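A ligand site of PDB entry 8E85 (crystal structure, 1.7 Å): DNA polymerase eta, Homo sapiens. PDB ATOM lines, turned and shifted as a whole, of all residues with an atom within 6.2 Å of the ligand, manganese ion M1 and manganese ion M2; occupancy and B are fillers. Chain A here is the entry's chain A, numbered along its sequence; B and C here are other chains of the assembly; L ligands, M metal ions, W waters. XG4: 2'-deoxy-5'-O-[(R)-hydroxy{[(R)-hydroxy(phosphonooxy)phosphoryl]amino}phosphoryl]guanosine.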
ATOM      1  N   ASP A  16      11.904  -4.072  36.708  1.00  0.00           N
ATOM      2  CA  ASP A  16      12.729  -4.241  35.489  1.00  0.00           C
ATOM      3  C   ASP A  16      11.930  -4.739  34.302  1.00  0.00           C
ATOM      4  O   ASP A  16      11.282  -5.797  34.384  1.00  0.00           O
ATOM      5  CB  ASP A  16      13.829  -5.279  35.719  1.00  0.00           C
ATOM      6  CG  ASP A  16      14.921  -5.190  34.705  1.00  0.00           C
ATOM      7  OD1 ASP A  16      15.899  -4.417  34.750  1.00  0.00           O
ATOM      8  OD2 ASP A  16      14.651  -5.898  33.726  1.00  0.00           O
ATOM      9  N   MET A  17      12.028  -4.052  33.163  1.00  0.00           N
ATOM     10  CA  MET A  17      11.191  -4.447  32.028  1.00  0.00           C
ATOM     11  C   MET A  17      11.688  -5.757  31.449  1.00  0.00           C
ATOM     12  O   MET A  17      12.887  -5.998  31.394  1.00  0.00           O
ATOM     13  CB  MET A  17      11.182  -3.362  30.946  1.00  0.00           C
ATOM     14  CG  MET A  17      10.922  -1.997  31.532  1.00  0.00           C
ATOM     15  SD  MET A  17       9.234  -1.895  32.243  1.00  0.00           S
ATOM     16  CE  MET A  17       8.238  -2.493  30.886  1.00  0.00           C
ATOM     17  N   ASP A  18      10.743  -6.620  31.042  1.00  0.00           N
ATOM     18  CA  ASP A  18      11.133  -7.878  30.389  1.00  0.00           C
ATOM     19  C   ASP A  18      11.611  -7.592  28.973  1.00  0.00           C
ATOM     20  O   ASP A  18      10.956  -6.851  28.234  1.00  0.00           O
ATOM     21  CB  ASP A  18       9.966  -8.879  30.339  1.00  0.00           C
ATOM     22  CG  ASP A  18       9.448  -9.274  31.726  1.00  0.00           C
ATOM     23  OD1 ASP A  18      10.284  -9.257  32.661  1.00  0.00           O
ATOM     24  OD2 ASP A  18       8.274  -9.675  31.849  1.00  0.00           O
ATOM     25  N   CYS A  19      12.692  -8.252  28.591  1.00  0.00           N
ATOM     26  CA  CYS A  19      13.380  -8.062  27.298  1.00  0.00           C
ATOM     27  C   CYS A  19      13.054  -6.721  26.648  1.00  0.00           C
ATOM     28  O   CYS A  19      12.418  -6.663  25.599  1.00  0.00           O
ATOM     29  CB  CYS A  19      13.035  -9.207  26.314  1.00  0.00           C
ATOM     30  SG  CYS A  19      11.333  -9.717  26.112  1.00  0.00           S
ATOM     31  N   PHE A  20      13.484  -5.635  27.282  1.00  0.00           N
ATOM     32  CA  PHE A  20      12.863  -4.321  27.058  1.00  0.00           C
ATOM     33  C   PHE A  20      12.877  -3.893  25.590  1.00  0.00           C
ATOM     34  O   PHE A  20      11.825  -3.544  25.027  1.00  0.00           O
ATOM     35  CB  PHE A  20      13.525  -3.270  27.938  1.00  0.00           C
ATOM     36  CG  PHE A  20      12.884  -1.917  27.812  1.00  0.00           C
ATOM     37  CD1 PHE A  20      11.504  -1.779  27.849  1.00  0.00           C
ATOM     38  CD2 PHE A  20      13.657  -0.782  27.723  1.00  0.00           C
ATOM     39  CE1 PHE A  20      10.896  -0.538  27.730  1.00  0.00           C
ATOM     40  CE2 PHE A  20      13.046   0.483  27.626  1.00  0.00           C
ATOM     41  CZ  PHE A  20      11.677   0.591  27.631  1.00  0.00           C
ATOM     42  N   PHE A  21      14.060  -3.830  24.954  1.00  0.00           N
ATOM     43  CA  PHE A  21      14.076  -3.305  23.587  1.00  0.00           C
ATOM     44  C   PHE A  21      13.273  -4.185  22.642  1.00  0.00           C
ATOM     45  O   PHE A  21      12.643  -3.685  21.696  1.00  0.00           O
ATOM     46  CB  PHE A  21      15.514  -3.149  23.054  1.00  0.00           C
ATOM     47  CG  PHE A  21      16.323  -2.019  23.668  1.00  0.00           C
ATOM     48  CD1 PHE A  21      16.008  -1.449  24.898  1.00  0.00           C
ATOM     49  CD2 PHE A  21      17.461  -1.574  23.019  1.00  0.00           C
ATOM     50  CE1 PHE A  21      16.805  -0.418  25.443  1.00  0.00           C
ATOM     51  CE2 PHE A  21      18.244  -0.552  23.549  1.00  0.00           C
ATOM     52  CZ  PHE A  21      17.918   0.021  24.760  1.00  0.00           C
ATOM     53  N   VAL A  22      13.266  -5.505  22.877  1.00  0.00           N
ATOM     54  CA  VAL A  22      12.393  -6.398  22.086  1.00  0.00           C
ATOM     55  C   VAL A  22      10.938  -6.010  22.261  1.00  0.00           C
ATOM     56  O   VAL A  22      10.173  -5.978  21.293  1.00  0.00           O
ATOM     57  CB  VAL A  22      12.629  -7.868  22.466  1.00  0.00           C
ATOM     58  CG1 VAL A  22      11.501  -8.752  21.885  1.00  0.00           C
ATOM     59  CG2 VAL A  22      13.970  -8.291  21.948  1.00  0.00           C
ATOM     60  N   GLN A  41      22.407  -4.107  16.957  1.00  0.00           N
ATOM     61  CA  GLN A  41      23.024  -2.851  16.546  1.00  0.00           C
ATOM     62  C   GLN A  41      23.943  -3.141  15.371  1.00  0.00           C
ATOM     63  O   GLN A  41      24.794  -4.033  15.464  1.00  0.00           O
ATOM     64  CB  GLN A  41      23.822  -2.212  17.697  1.00  0.00           C
ATOM     65  CG  GLN A  41      22.968  -1.747  18.845  1.00  0.00           C
ATOM     66  CD  GLN A  41      23.766  -1.002  19.904  1.00  0.00           C
ATOM     67  OE1 GLN A  41      23.355   0.071  20.347  1.00  0.00           O
ATOM     68  NE2 GLN A  41      24.849  -1.622  20.394  1.00  0.00           N
ATOM     69  N   ILE A  51      21.601  -7.080  21.537  1.00  0.00           N
ATOM     70  CA  ILE A  51      21.571  -6.472  22.863  1.00  0.00           C
ATOM     71  C   ILE A  51      20.324  -6.822  23.668  1.00  0.00           C
ATOM     72  O   ILE A  51      20.264  -6.505  24.869  1.00  0.00           O
ATOM     73  CB  ILE A  51      21.741  -4.940  22.792  1.00  0.00           C
ATOM     74  CG1 ILE A  51      20.709  -4.304  21.861  1.00  0.00           C
ATOM     75  CG2 ILE A  51      23.159  -4.581  22.319  1.00  0.00           C
ATOM     76  CD1 ILE A  51      20.738  -2.767  21.905  1.00  0.00           C
ATOM     77  N   ALA A  52      19.324  -7.486  23.073  1.00  0.00           N
ATOM     78  CA  ALA A  52      18.082  -7.867  23.748  1.00  0.00           C
ATOM     79  C   ALA A  52      17.455  -9.060  23.031  1.00  0.00           C
ATOM     80  O   ALA A  52      17.489  -9.118  21.809  1.00  0.00           O
ATOM     81  CB  ALA A  52      17.077  -6.725  23.765  1.00  0.00           C
ATOM     82  N   VAL A  53      16.885  -9.990  23.805  1.00  0.00           N
ATOM     83  CA  VAL A  53      16.432 -11.295  23.296  1.00  0.00           C
ATOM     84  C   VAL A  53      15.107 -11.646  23.915  1.00  0.00           C
ATOM     85  O   VAL A  53      14.980 -11.648  25.150  1.00  0.00           O
ATOM     86  CB  VAL A  53      17.455 -12.399  23.638  1.00  0.00           C
ATOM     87  CG1 VAL A  53      17.100 -13.686  22.917  1.00  0.00           C
ATOM     88  CG2 VAL A  53      18.817 -11.978  23.262  1.00  0.00           C
ATOM     89  N   TYR A  55      12.032 -14.069  25.246  1.00  0.00           N
ATOM     90  CA  TYR A  55      12.187 -15.291  26.033  1.00  0.00           C
ATOM     91  C   TYR A  55      12.008 -16.541  25.164  1.00  0.00           C
ATOM     92  O   TYR A  55      12.675 -17.569  25.403  1.00  0.00           O
ATOM     93  CB  TYR A  55      11.240 -15.245  27.238  1.00  0.00           C
ATOM     94  CG  TYR A  55      11.806 -14.368  28.347  1.00  0.00           C
ATOM     95  CD1 TYR A  55      11.777 -12.983  28.251  1.00  0.00           C
ATOM     96  CD2 TYR A  55      12.476 -14.936  29.430  1.00  0.00           C
ATOM     97  CE1 TYR A  55      12.317 -12.172  29.243  1.00  0.00           C
ATOM     98  CE2 TYR A  55      13.033 -14.139  30.415  1.00  0.00           C
ATOM     99  CZ  TYR A  55      12.962 -12.757  30.327  1.00  0.00           C
ATOM    100  OH  TYR A  55      13.542 -11.987  31.314  1.00  0.00           O
ATOM    101  N   ARG A  58      15.403 -17.019  23.828  1.00  0.00           N
ATOM    102  CA  ARG A  58      16.332 -17.483  24.852  1.00  0.00           C
ATOM    103  C   ARG A  58      16.273 -18.989  25.025  1.00  0.00           C
ATOM    104  O   ARG A  58      17.297 -19.609  25.371  1.00  0.00           O
ATOM    105  CB  ARG A  58      16.064 -16.795  26.185  1.00  0.00           C
ATOM    106  CG  ARG A  58      16.370 -15.322  26.165  1.00  0.00           C
ATOM    107  CD  ARG A  58      16.066 -14.740  27.500  1.00  0.00           C
ATOM    108  NE  ARG A  58      15.897 -13.306  27.411  1.00  0.00           N
ATOM    109  CZ  ARG A  58      15.933 -12.496  28.462  1.00  0.00           C
ATOM    110  NH1 ARG A  58      16.169 -12.964  29.677  1.00  0.00           N
ATOM    111  NH2 ARG A  58      15.751 -11.193  28.272  1.00  0.00           N
ATOM    112  N   ARG A  64      22.433 -12.002  24.841  1.00  0.00           N
ATOM    113  CA  ARG A  64      23.019 -10.684  24.544  1.00  0.00           C
ATOM    114  C   ARG A  64      24.501 -10.921  24.292  1.00  0.00           C
ATOM    115  O   ARG A  64      25.025 -11.891  24.841  1.00  0.00           O
ATOM    116  CB  ARG A  64      22.752  -9.764  25.730  1.00  0.00           C
ATOM    117  CG  ARG A  64      23.842  -8.750  26.048  1.00  0.00           C
ATOM    118  CD  ARG A  64      23.544  -8.050  27.354  1.00  0.00           C
ATOM    119  NE  ARG A  64      24.379  -6.871  27.474  1.00  0.00           N
ATOM    120  CZ  ARG A  64      25.619  -6.871  27.932  1.00  0.00           C
ATOM    121  NH1 ARG A  64      26.167  -7.994  28.344  1.00  0.00           N
ATOM    122  NH2 ARG A  64      26.311  -5.746  27.979  1.00  0.00           N
ATOM    123  N   SER A  65      25.121 -10.070  23.501  1.00  0.00           N
ATOM    124  CA  SER A  65      26.581 -10.149  23.207  1.00  0.00           C
ATOM    125  C   SER A  65      26.841 -11.233  22.157  1.00  0.00           C
ATOM    126  O   SER A  65      28.009 -11.492  21.902  1.00  0.00           O
ATOM    127  CB  SER A  65      27.411 -10.326  24.436  1.00  0.00           C
ATOM    128  OG  SER A  65      27.205  -9.228  25.319  1.00  0.00           O
ATOM    129  N   LEU A  92      19.662   5.394  20.173  1.00  0.00           N
ATOM    130  CA  LEU A  92      18.782   4.677  21.088  1.00  0.00           C
ATOM    131  C   LEU A  92      17.560   5.498  21.531  1.00  0.00           C
ATOM    132  O   LEU A  92      16.877   5.133  22.506  1.00  0.00           O
ATOM    133  CB  LEU A  92      19.583   4.191  22.315  1.00  0.00           C
ATOM    134  CG  LEU A  92      20.838   3.380  21.965  1.00  0.00           C
ATOM    135  CD1 LEU A  92      21.684   3.067  23.190  1.00  0.00           C
ATOM    136  CD2 LEU A  92      20.394   2.095  21.302  1.00  0.00           C
ATOM    137  N   SER A 116      18.427   2.261  35.456  1.00  0.00           N
ATOM    138  CA  SER A 116      18.933   2.026  34.102  1.00  0.00           C
ATOM    139  C   SER A 116      17.828   2.438  33.141  1.00  0.00           C
ATOM    140  O   SER A 116      16.710   2.756  33.552  1.00  0.00           O
ATOM    141  CB  SER A 116      19.294   0.567  33.880  1.00  0.00           C
ATOM    142  OG  SER A 116      18.082  -0.157  33.608  1.00  0.00           O
ATOM    143  N   ILE A 117      18.110   2.276  31.828  1.00  0.00           N
ATOM    144  CA  ILE A 117      17.118   2.604  30.811  1.00  0.00           C
ATOM    145  C   ILE A 117      15.809   1.852  31.048  1.00  0.00           C
ATOM    146  O   ILE A 117      14.756   2.334  30.641  1.00  0.00           O
ATOM    147  CB  ILE A 117      17.635   2.319  29.389  1.00  0.00           C
ATOM    148  CG1 ILE A 117      16.722   3.006  28.355  1.00  0.00           C
ATOM    149  CG2 ILE A 117      17.669   0.792  29.132  1.00  0.00           C
ATOM    150  CD1 ILE A 117      17.366   3.189  26.950  1.00  0.00           C
ATOM    151  N   ASP A 118      15.843   0.694  31.745  1.00  0.00           N
ATOM    152  CA  ASP A 118      14.598  -0.081  31.804  1.00  0.00           C
ATOM    153  C   ASP A 118      14.252  -0.482  33.241  1.00  0.00           C
ATOM    154  O   ASP A 118      13.489  -1.438  33.451  1.00  0.00           O
ATOM    155  CB  ASP A 118      14.675  -1.344  30.934  1.00  0.00           C
ATOM    156  CG  ASP A 118      15.268  -2.562  31.670  1.00  0.00           C
ATOM    157  OD1 ASP A 118      16.247  -2.432  32.432  1.00  0.00           O
ATOM    158  OD2 ASP A 118      14.703  -3.667  31.458  1.00  0.00           O
ATOM    159  N   GLU A 119      14.821   0.181  34.247  1.00  0.00           N
ATOM    160  CA  GLU A 119      14.538  -0.268  35.612  1.00  0.00           C
ATOM    161  C   GLU A 119      14.623   0.877  36.601  1.00  0.00           C
ATOM    162  O   GLU A 119      15.401   1.826  36.423  1.00  0.00           O
ATOM    163  CB  GLU A 119      15.413  -1.448  36.010  1.00  0.00           C
ATOM    164  CG  GLU A 119      16.792  -1.029  36.417  1.00  0.00           C
ATOM    165  CD  GLU A 119      17.769  -2.167  36.265  1.00  0.00           C
ATOM    166  OE1 GLU A 119      17.890  -2.993  37.198  1.00  0.00           O
ATOM    167  OE2 GLU A 119      18.176  -2.403  35.106  1.00  0.00           O
ATOM    168  N   LYS A 227      16.520  -6.116  43.804  1.00  0.00           N
ATOM    169  CA  LYS A 227      17.064  -6.417  42.484  1.00  0.00           C
ATOM    170  C   LYS A 227      17.265  -7.911  42.318  1.00  0.00           C
ATOM    171  O   LYS A 227      16.941  -8.475  41.255  1.00  0.00           O
ATOM    172  CB  LYS A 227      18.385  -5.663  42.282  1.00  0.00           C
ATOM    173  CG  LYS A 227      19.124  -6.021  41.016  1.00  0.00           C
ATOM    174  CD  LYS A 227      18.359  -5.629  39.742  1.00  0.00           C
ATOM    175  CE  LYS A 227      19.266  -5.823  38.528  1.00  0.00           C
ATOM    176  NZ  LYS A 227      18.597  -5.571  37.224  1.00  0.00           N
ATOM    177  N   LYS A 234      11.571 -14.048  36.499  1.00  0.00           N
ATOM    178  CA  LYS A 234      11.301 -13.418  35.224  1.00  0.00           C
ATOM    179  C   LYS A 234      10.944 -14.505  34.221  1.00  0.00           C
ATOM    180  O   LYS A 234      11.509 -15.606  34.275  1.00  0.00           O
ATOM    181  CB  LYS A 234      12.534 -12.670  34.710  1.00  0.00           C
ATOM    182  CG  LYS A 234      12.571 -11.249  35.148  1.00  0.00           C
ATOM    183  CD  LYS A 234      13.631 -10.443  34.427  1.00  0.00           C
ATOM    184  CE  LYS A 234      13.268  -8.992  34.670  1.00  0.00           C
ATOM    185  NZ  LYS A 234      12.914  -8.284  33.427  1.00  0.00           N
ATOM    186  N   PRO A 235      10.065 -14.209  33.253  1.00  0.00           N
ATOM    187  CA  PRO A 235       9.418 -12.923  32.997  1.00  0.00           C
ATOM    188  C   PRO A 235       8.007 -12.798  33.517  1.00  0.00           C
ATOM    189  O   PRO A 235       7.341 -13.814  33.817  1.00  0.00           O
ATOM    190  CB  PRO A 235       9.408 -12.880  31.467  1.00  0.00           C
ATOM    191  CG  PRO A 235       9.086 -14.308  31.105  1.00  0.00           C
ATOM    192  CD  PRO A 235       9.777 -15.166  32.165  1.00  0.00           C
ATOM    193  P     G B   8      22.702  -6.035  35.846  1.00  0.00           P
ATOM    194  OP1   G B   8      21.414  -5.619  35.167  1.00  0.00           O
ATOM    195  OP2   G B   8      22.514  -7.044  36.948  1.00  0.00           O
ATOM    196  O5'   G B   8      23.679  -6.716  34.754  1.00  0.00           O
ATOM    197  C5'   G B   8      23.157  -7.168  33.466  1.00  0.00           C
ATOM    198  C4'   G B   8      22.826  -5.972  32.598  1.00  0.00           C
ATOM    199  O4'   G B   8      23.788  -4.908  32.800  1.00  0.00           O
ATOM    200  C3'   G B   8      22.902  -6.169  31.074  1.00  0.00           C
ATOM    201  O3'   G B   8      21.833  -6.948  30.545  1.00  0.00           O
ATOM    202  C2'   G B   8      22.805  -4.701  30.670  1.00  0.00           C
ATOM    203  O2'   G B   8      21.506  -4.177  30.809  1.00  0.00           O
ATOM    204  C1'   G B   8      23.782  -4.065  31.667  1.00  0.00           C
ATOM    205  N9    G B   8      25.122  -3.960  31.120  1.00  0.00           N
ATOM    206  C8    G B   8      26.219  -4.735  31.399  1.00  0.00           C
ATOM    207  N7    G B   8      27.279  -4.403  30.707  1.00  0.00           N
ATOM    208  C5    G B   8      26.845  -3.351  29.905  1.00  0.00           C
ATOM    209  C6    G B   8      27.539  -2.587  28.939  1.00  0.00           C
ATOM    210  O6    G B   8      28.729  -2.682  28.596  1.00  0.00           O
ATOM    211  N1    G B   8      26.715  -1.618  28.366  1.00  0.00           N
ATOM    212  C2    G B   8      25.394  -1.422  28.669  1.00  0.00           C
ATOM    213  N2    G B   8      24.762  -0.449  27.995  1.00  0.00           N
ATOM    214  N3    G B   8      24.734  -2.135  29.566  1.00  0.00           N
ATOM    215  C4    G B   8      25.514  -3.074  30.149  1.00  0.00           C
ATOM    216  P    DT C   4      32.516  -4.376  19.625  1.00  0.00           P
ATOM    217  OP1  DT C   4      33.039  -4.223  18.253  1.00  0.00           O
ATOM    218  OP2  DT C   4      33.387  -4.159  20.801  1.00  0.00           O
ATOM    219  O5'  DT C   4      31.273  -3.366  19.741  1.00  0.00           O
ATOM    220  C5'  DT C   4      30.340  -3.280  18.646  1.00  0.00           C
ATOM    221  C4'  DT C   4      29.227  -2.332  19.016  1.00  0.00           C
ATOM    222  O4'  DT C   4      28.526  -2.827  20.177  1.00  0.00           O
ATOM    223  C3'  DT C   4      29.671  -0.917  19.377  1.00  0.00           C
ATOM    224  O3'  DT C   4      28.656  -0.034  18.959  1.00  0.00           O
ATOM    225  C2'  DT C   4      29.752  -0.981  20.893  1.00  0.00           C
ATOM    226  C1'  DT C   4      28.559  -1.861  21.212  1.00  0.00           C
ATOM    227  N1   DT C   4      28.635  -2.593  22.488  1.00  0.00           N
ATOM    228  C2   DT C   4      27.521  -2.578  23.302  1.00  0.00           C
ATOM    229  O2   DT C   4      26.503  -1.977  23.017  1.00  0.00           O
ATOM    230  N3   DT C   4      27.653  -3.302  24.462  1.00  0.00           N
ATOM    231  C4   DT C   4      28.767  -4.018  24.874  1.00  0.00           C
ATOM    232  O4   DT C   4      28.737  -4.613  25.948  1.00  0.00           O
ATOM    233  C5   DT C   4      29.892  -3.990  23.971  1.00  0.00           C
ATOM    234  C7   DT C   4      31.131  -4.735  24.363  1.00  0.00           C
ATOM    235  C6   DT C   4      29.769  -3.283  22.834  1.00  0.00           C
ATOM    236  P    DC C   5      28.958   1.518  19.224  1.00  0.00           P
ATOM    237  OP1  DC C   5      28.577   2.343  18.033  1.00  0.00           O
ATOM    238  OP2  DC C   5      30.332   1.779  19.746  1.00  0.00           O
ATOM    239  O5'  DC C   5      27.927   1.866  20.402  1.00  0.00           O
ATOM    240  C5'  DC C   5      26.511   1.685  20.166  1.00  0.00           C
ATOM    241  C4'  DC C   5      25.736   2.177  21.357  1.00  0.00           C
ATOM    242  O4'  DC C   5      25.938   1.269  22.474  1.00  0.00           O
ATOM    243  C3'  DC C   5      26.152   3.559  21.865  1.00  0.00           C
ATOM    244  O3'  DC C   5      24.984   4.200  22.374  1.00  0.00           O
ATOM    245  C2'  DC C   5      27.118   3.222  22.989  1.00  0.00           C
ATOM    246  C1'  DC C   5      26.455   1.976  23.570  1.00  0.00           C
ATOM    247  N1   DC C   5      27.372   1.074  24.305  1.00  0.00           N
ATOM    248  C2   DC C   5      26.890   0.427  25.436  1.00  0.00           C
ATOM    249  O2   DC C   5      25.729   0.634  25.788  1.00  0.00           O
ATOM    250  N3   DC C   5      27.712  -0.404  26.114  1.00  0.00           N
ATOM    251  C4   DC C   5      28.968  -0.588  25.694  1.00  0.00           C
ATOM    252  N4   DC C   5      29.732  -1.410  26.402  1.00  0.00           N
ATOM    253  C5   DC C   5      29.476   0.062  24.543  1.00  0.00           C
ATOM    254  C6   DC C   5      28.647   0.876  23.877  1.00  0.00           C
ATOM    255  P    DT C   6      25.147   5.771  22.644  1.00  0.00           P
ATOM    256  OP1  DT C   6      23.818   6.356  23.002  1.00  0.00           O
ATOM    257  OP2  DT C   6      25.857   6.488  21.535  1.00  0.00           O
ATOM    258  O5'  DT C   6      26.099   5.813  23.920  1.00  0.00           O
ATOM    259  C5'  DT C   6      25.636   6.466  25.115  1.00  0.00           C
ATOM    260  C4'  DT C   6      24.957   5.458  26.012  1.00  0.00           C
ATOM    261  O4'  DT C   6      25.804   4.306  26.170  1.00  0.00           O
ATOM    262  C3'  DT C   6      24.680   5.981  27.415  1.00  0.00           C
ATOM    263  O3'  DT C   6      23.320   6.403  27.488  1.00  0.00           O
ATOM    264  C2'  DT C   6      24.983   4.803  28.339  1.00  0.00           C
ATOM    265  C1'  DT C   6      25.506   3.697  27.420  1.00  0.00           C
ATOM    266  N1   DT C   6      26.722   3.012  27.877  1.00  0.00           N
ATOM    267  C2   DT C   6      26.641   2.164  28.961  1.00  0.00           C
ATOM    268  O2   DT C   6      25.611   1.979  29.590  1.00  0.00           O
ATOM    269  N3   DT C   6      27.820   1.543  29.294  1.00  0.00           N
ATOM    270  C4   DT C   6      29.038   1.668  28.660  1.00  0.00           C
ATOM    271  O4   DT C   6      30.014   1.047  29.076  1.00  0.00           O
ATOM    272  C5   DT C   6      29.055   2.560  27.527  1.00  0.00           C
ATOM    273  C7   DT C   6      30.336   2.769  26.781  1.00  0.00           C
ATOM    274  C6   DT C   6      27.913   3.179  27.193  1.00  0.00           C
HETATM  275  N1  XG4 L   1      24.403  -2.125  24.853  1.00  0.00           N
HETATM  276  C2  XG4 L   1      23.286  -1.390  24.515  1.00  0.00           C
HETATM  277  N2  XG4 L   1      23.475  -0.406  23.624  1.00  0.00           N
HETATM  278  N3  XG4 L   1      22.077  -1.610  25.017  1.00  0.00           N
HETATM  279  C4  XG4 L   1      22.079  -2.642  25.897  1.00  0.00           C
HETATM  280  C5  XG4 L   1      23.129  -3.424  26.298  1.00  0.00           C
HETATM  281  C6  XG4 L   1      24.415  -3.183  25.755  1.00  0.00           C
HETATM  282  O6  XG4 L   1      25.467  -3.787  26.009  1.00  0.00           O
HETATM  283  N7  XG4 L   1      22.710  -4.367  27.222  1.00  0.00           N
HETATM  284  C8  XG4 L   1      21.425  -4.143  27.366  1.00  0.00           C
HETATM  285  N9  XG4 L   1      20.990  -3.108  26.583  1.00  0.00           N
HETATM  286  PA  XG4 L   1      18.322  -5.599  30.712  1.00  0.00           P
HETATM  287  PB  XG4 L   1      16.308  -6.978  29.069  1.00  0.00           P
HETATM  288  PG  XG4 L   1      15.447  -9.005  30.936  1.00  0.00           P
HETATM  289  C1' XG4 L   1      19.626  -2.608  26.483  1.00  0.00           C
HETATM  290  O1A XG4 L   1      17.235  -5.177  31.653  1.00  0.00           O
HETATM  291  O1B XG4 L   1      15.314  -6.012  29.635  1.00  0.00           O
HETATM  292  O1G XG4 L   1      15.601  -7.861  31.880  1.00  0.00           O
HETATM  293  C2' XG4 L   1      18.705  -3.597  25.782  1.00  0.00           C
HETATM  294  O2A XG4 L   1      19.646  -5.977  31.303  1.00  0.00           O
HETATM  295  O2B XG4 L   1      16.420  -7.080  27.577  1.00  0.00           O
HETATM  296  O2G XG4 L   1      14.024  -9.469  30.804  1.00  0.00           O
HETATM  297  C3' XG4 L   1      17.874  -4.192  26.922  1.00  0.00           C
HETATM  298  O3' XG4 L   1      16.569  -4.548  26.479  1.00  0.00           O
HETATM  299  N3A XG4 L   1      17.802  -6.767  29.701  1.00  0.00           N
HETATM  300  O3B XG4 L   1      15.858  -8.439  29.507  1.00  0.00           O
HETATM  301  O3G XG4 L   1      16.385 -10.123  31.225  1.00  0.00           O
HETATM  302  C4' XG4 L   1      17.829  -3.034  27.906  1.00  0.00           C
HETATM  303  O4' XG4 L   1      19.114  -2.394  27.794  1.00  0.00           O
HETATM  304  C5' XG4 L   1      17.595  -3.439  29.340  1.00  0.00           C
HETATM  305  O5' XG4 L   1      18.642  -4.344  29.782  1.00  0.00           O
HETATM  306 MN    MN M   1      15.065  -5.748  31.689  1.00  0.00          MN
HETATM  307 MN    MN M   2      17.484  -3.819  33.436  1.00  0.00          MN
HETATM  308  O   HOH W   1      18.835  -5.546  34.179  1.00  0.00           O
HETATM  309  O   HOH W   2      17.342  -7.747  34.086  1.00  0.00           O
HETATM  310  O   HOH W   3      17.254  -9.318  26.588  1.00  0.00           O
HETATM  311  O   HOH W   4      18.808 -10.542  30.639  1.00  0.00           O
HETATM  312  O   HOH W   5      19.763  -7.440  27.665  1.00  0.00           O
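Ser 116 touches manganese ion M2.
Four residues have an atom within 4 Å of manganese ion M2: Asp 16, Ser 116, Asp 118 and Glu 119.
Water W1 lies within hydrogen-bond range of OP1 of G 8 of chain B, O2A of the ligand and NZ of Lys 227.
Water W3 lies within hydrogen-bond range of O2B of the ligand (2.6 Å), N of Val 53 (2.9 Å) and NH2 of Arg 58 (2.9 Å).
Water W5 lies within hydrogen-bond range of N3A of the ligand (2.9 Å) and O of Ile 51 (3.0 Å).
The backbone carbonyl oxygen (O) of Asp 16 sits at hydrogen-bond distance from the side-chain amino group (NZ) of Lys 234 (3.1 Å).
NZ of Lys 234 sits close to O of Met 17, at 3.1 Å.
N of Glu 119 lies close to OG of Ser 116 (3.3 Å).
N7 of G 8 of chain B sits close to NH2 of Arg 64 (3.2 Å).
N2 of G 8 of chain B lies close to O2 of DC 5 of chain C (2.6 Å).
O2 of DT 4 of chain C sits at hydrogen-bond distance from the side-chain amide nitrogen (NE2) of Gln 41 (3.1 Å).
The guanidinium group (NE) of Arg 58 lies within hydrogen-bond range of the backbone carbonyl oxygen (O) of Val 53 (2.9 Å).
The side-chain amino group of Lys 234 lies within salt-bridge range of the side-chain carboxylate of Asp 18 (2.9 Å).
Merely in contact with manganese ion M1: Lys 234 (3.8 Å).
Of the 27 residues printed, 4 come within 4 Å of manganese ion M1.
The nearest printed residue that does not touch manganese ion M1 is Asp 18 (4.5 Å).
O3' of G 8 of chain B lies close to an oxygen (O2A) of the ligand (2.5 Å).
An oxygen (O2G) of the ligand sits at hydrogen-bond distance from the side-chain hydroxyl (OH) of Tyr 55, 2.6 Å away.
A nitrogen (N1) of the ligand lies within hydrogen-bond range of O2 of DT 4 of chain C (2.8 Å).
An oxygen (O2G) of the ligand is in hydrogen-bond range of the backbone NH (N) of Cys 19 (2.9 Å).
O6 of the ligand sits at hydrogen-bond distance from NH2 of Arg 64, at 2.9 Å.
The backbone NH of Phe 20 is in hydrogen-bond range of an oxygen (O2B) of the ligand (3.3 Å).
O3G of the ligand lies within salt-bridge range of NH2 of Arg 58, at 3.2 Å.
N of Phe 21 lies within hydrogen-bond range of O3' of the ligand (3.0 Å).
NZ of Lys 234 lies within salt-bridge range of O2G of the ligand (3.1 Å).
O4' of DC 5 of chain C lies within hydrogen-bond range of N2 of the ligand.
O2 of DC 5 of chain C sits at hydrogen-bond distance from N1 of the ligand, at 3.2 Å.
N2 of the ligand is in hydrogen-bond range of OE1 of Gln 41 (3.3 Å).
Manganese ion M2 is bound by the side-chain carboxylate (OD1) of Asp 118, the side-chain carboxylate (OD1) of Asp 16, an oxygen (O1A) of the ligand, the side-chain carboxylate (OE2) of Glu 119 and water W1.
Manganese ion M1 is bound by OD2 of Asp 16 (2.1 Å), O1B of the ligand (2.1 Å), OD2 of Asp 118 (2.1 Å), O1G of the ligand (2.2 Å), O of Met 17 (2.2 Å) and O1A of the ligand (2.2 Å).
Residues that only touch the ligand: Asp 18 (3.3 Å), Ile 51 (3.4 Å), Ala 52 (3.5 Å), Ile 117 (3.7 Å) and Leu 92 (3.9 Å).
Hydrophobic or aromatic side chains within 4 Å of the ligand: Phe 20, Phe 21, Ile 51, Ala 52, Tyr 55, Leu 92 and Ile 117.
Of the 27 residues printed, 19 come within 4 Å of the ligand.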
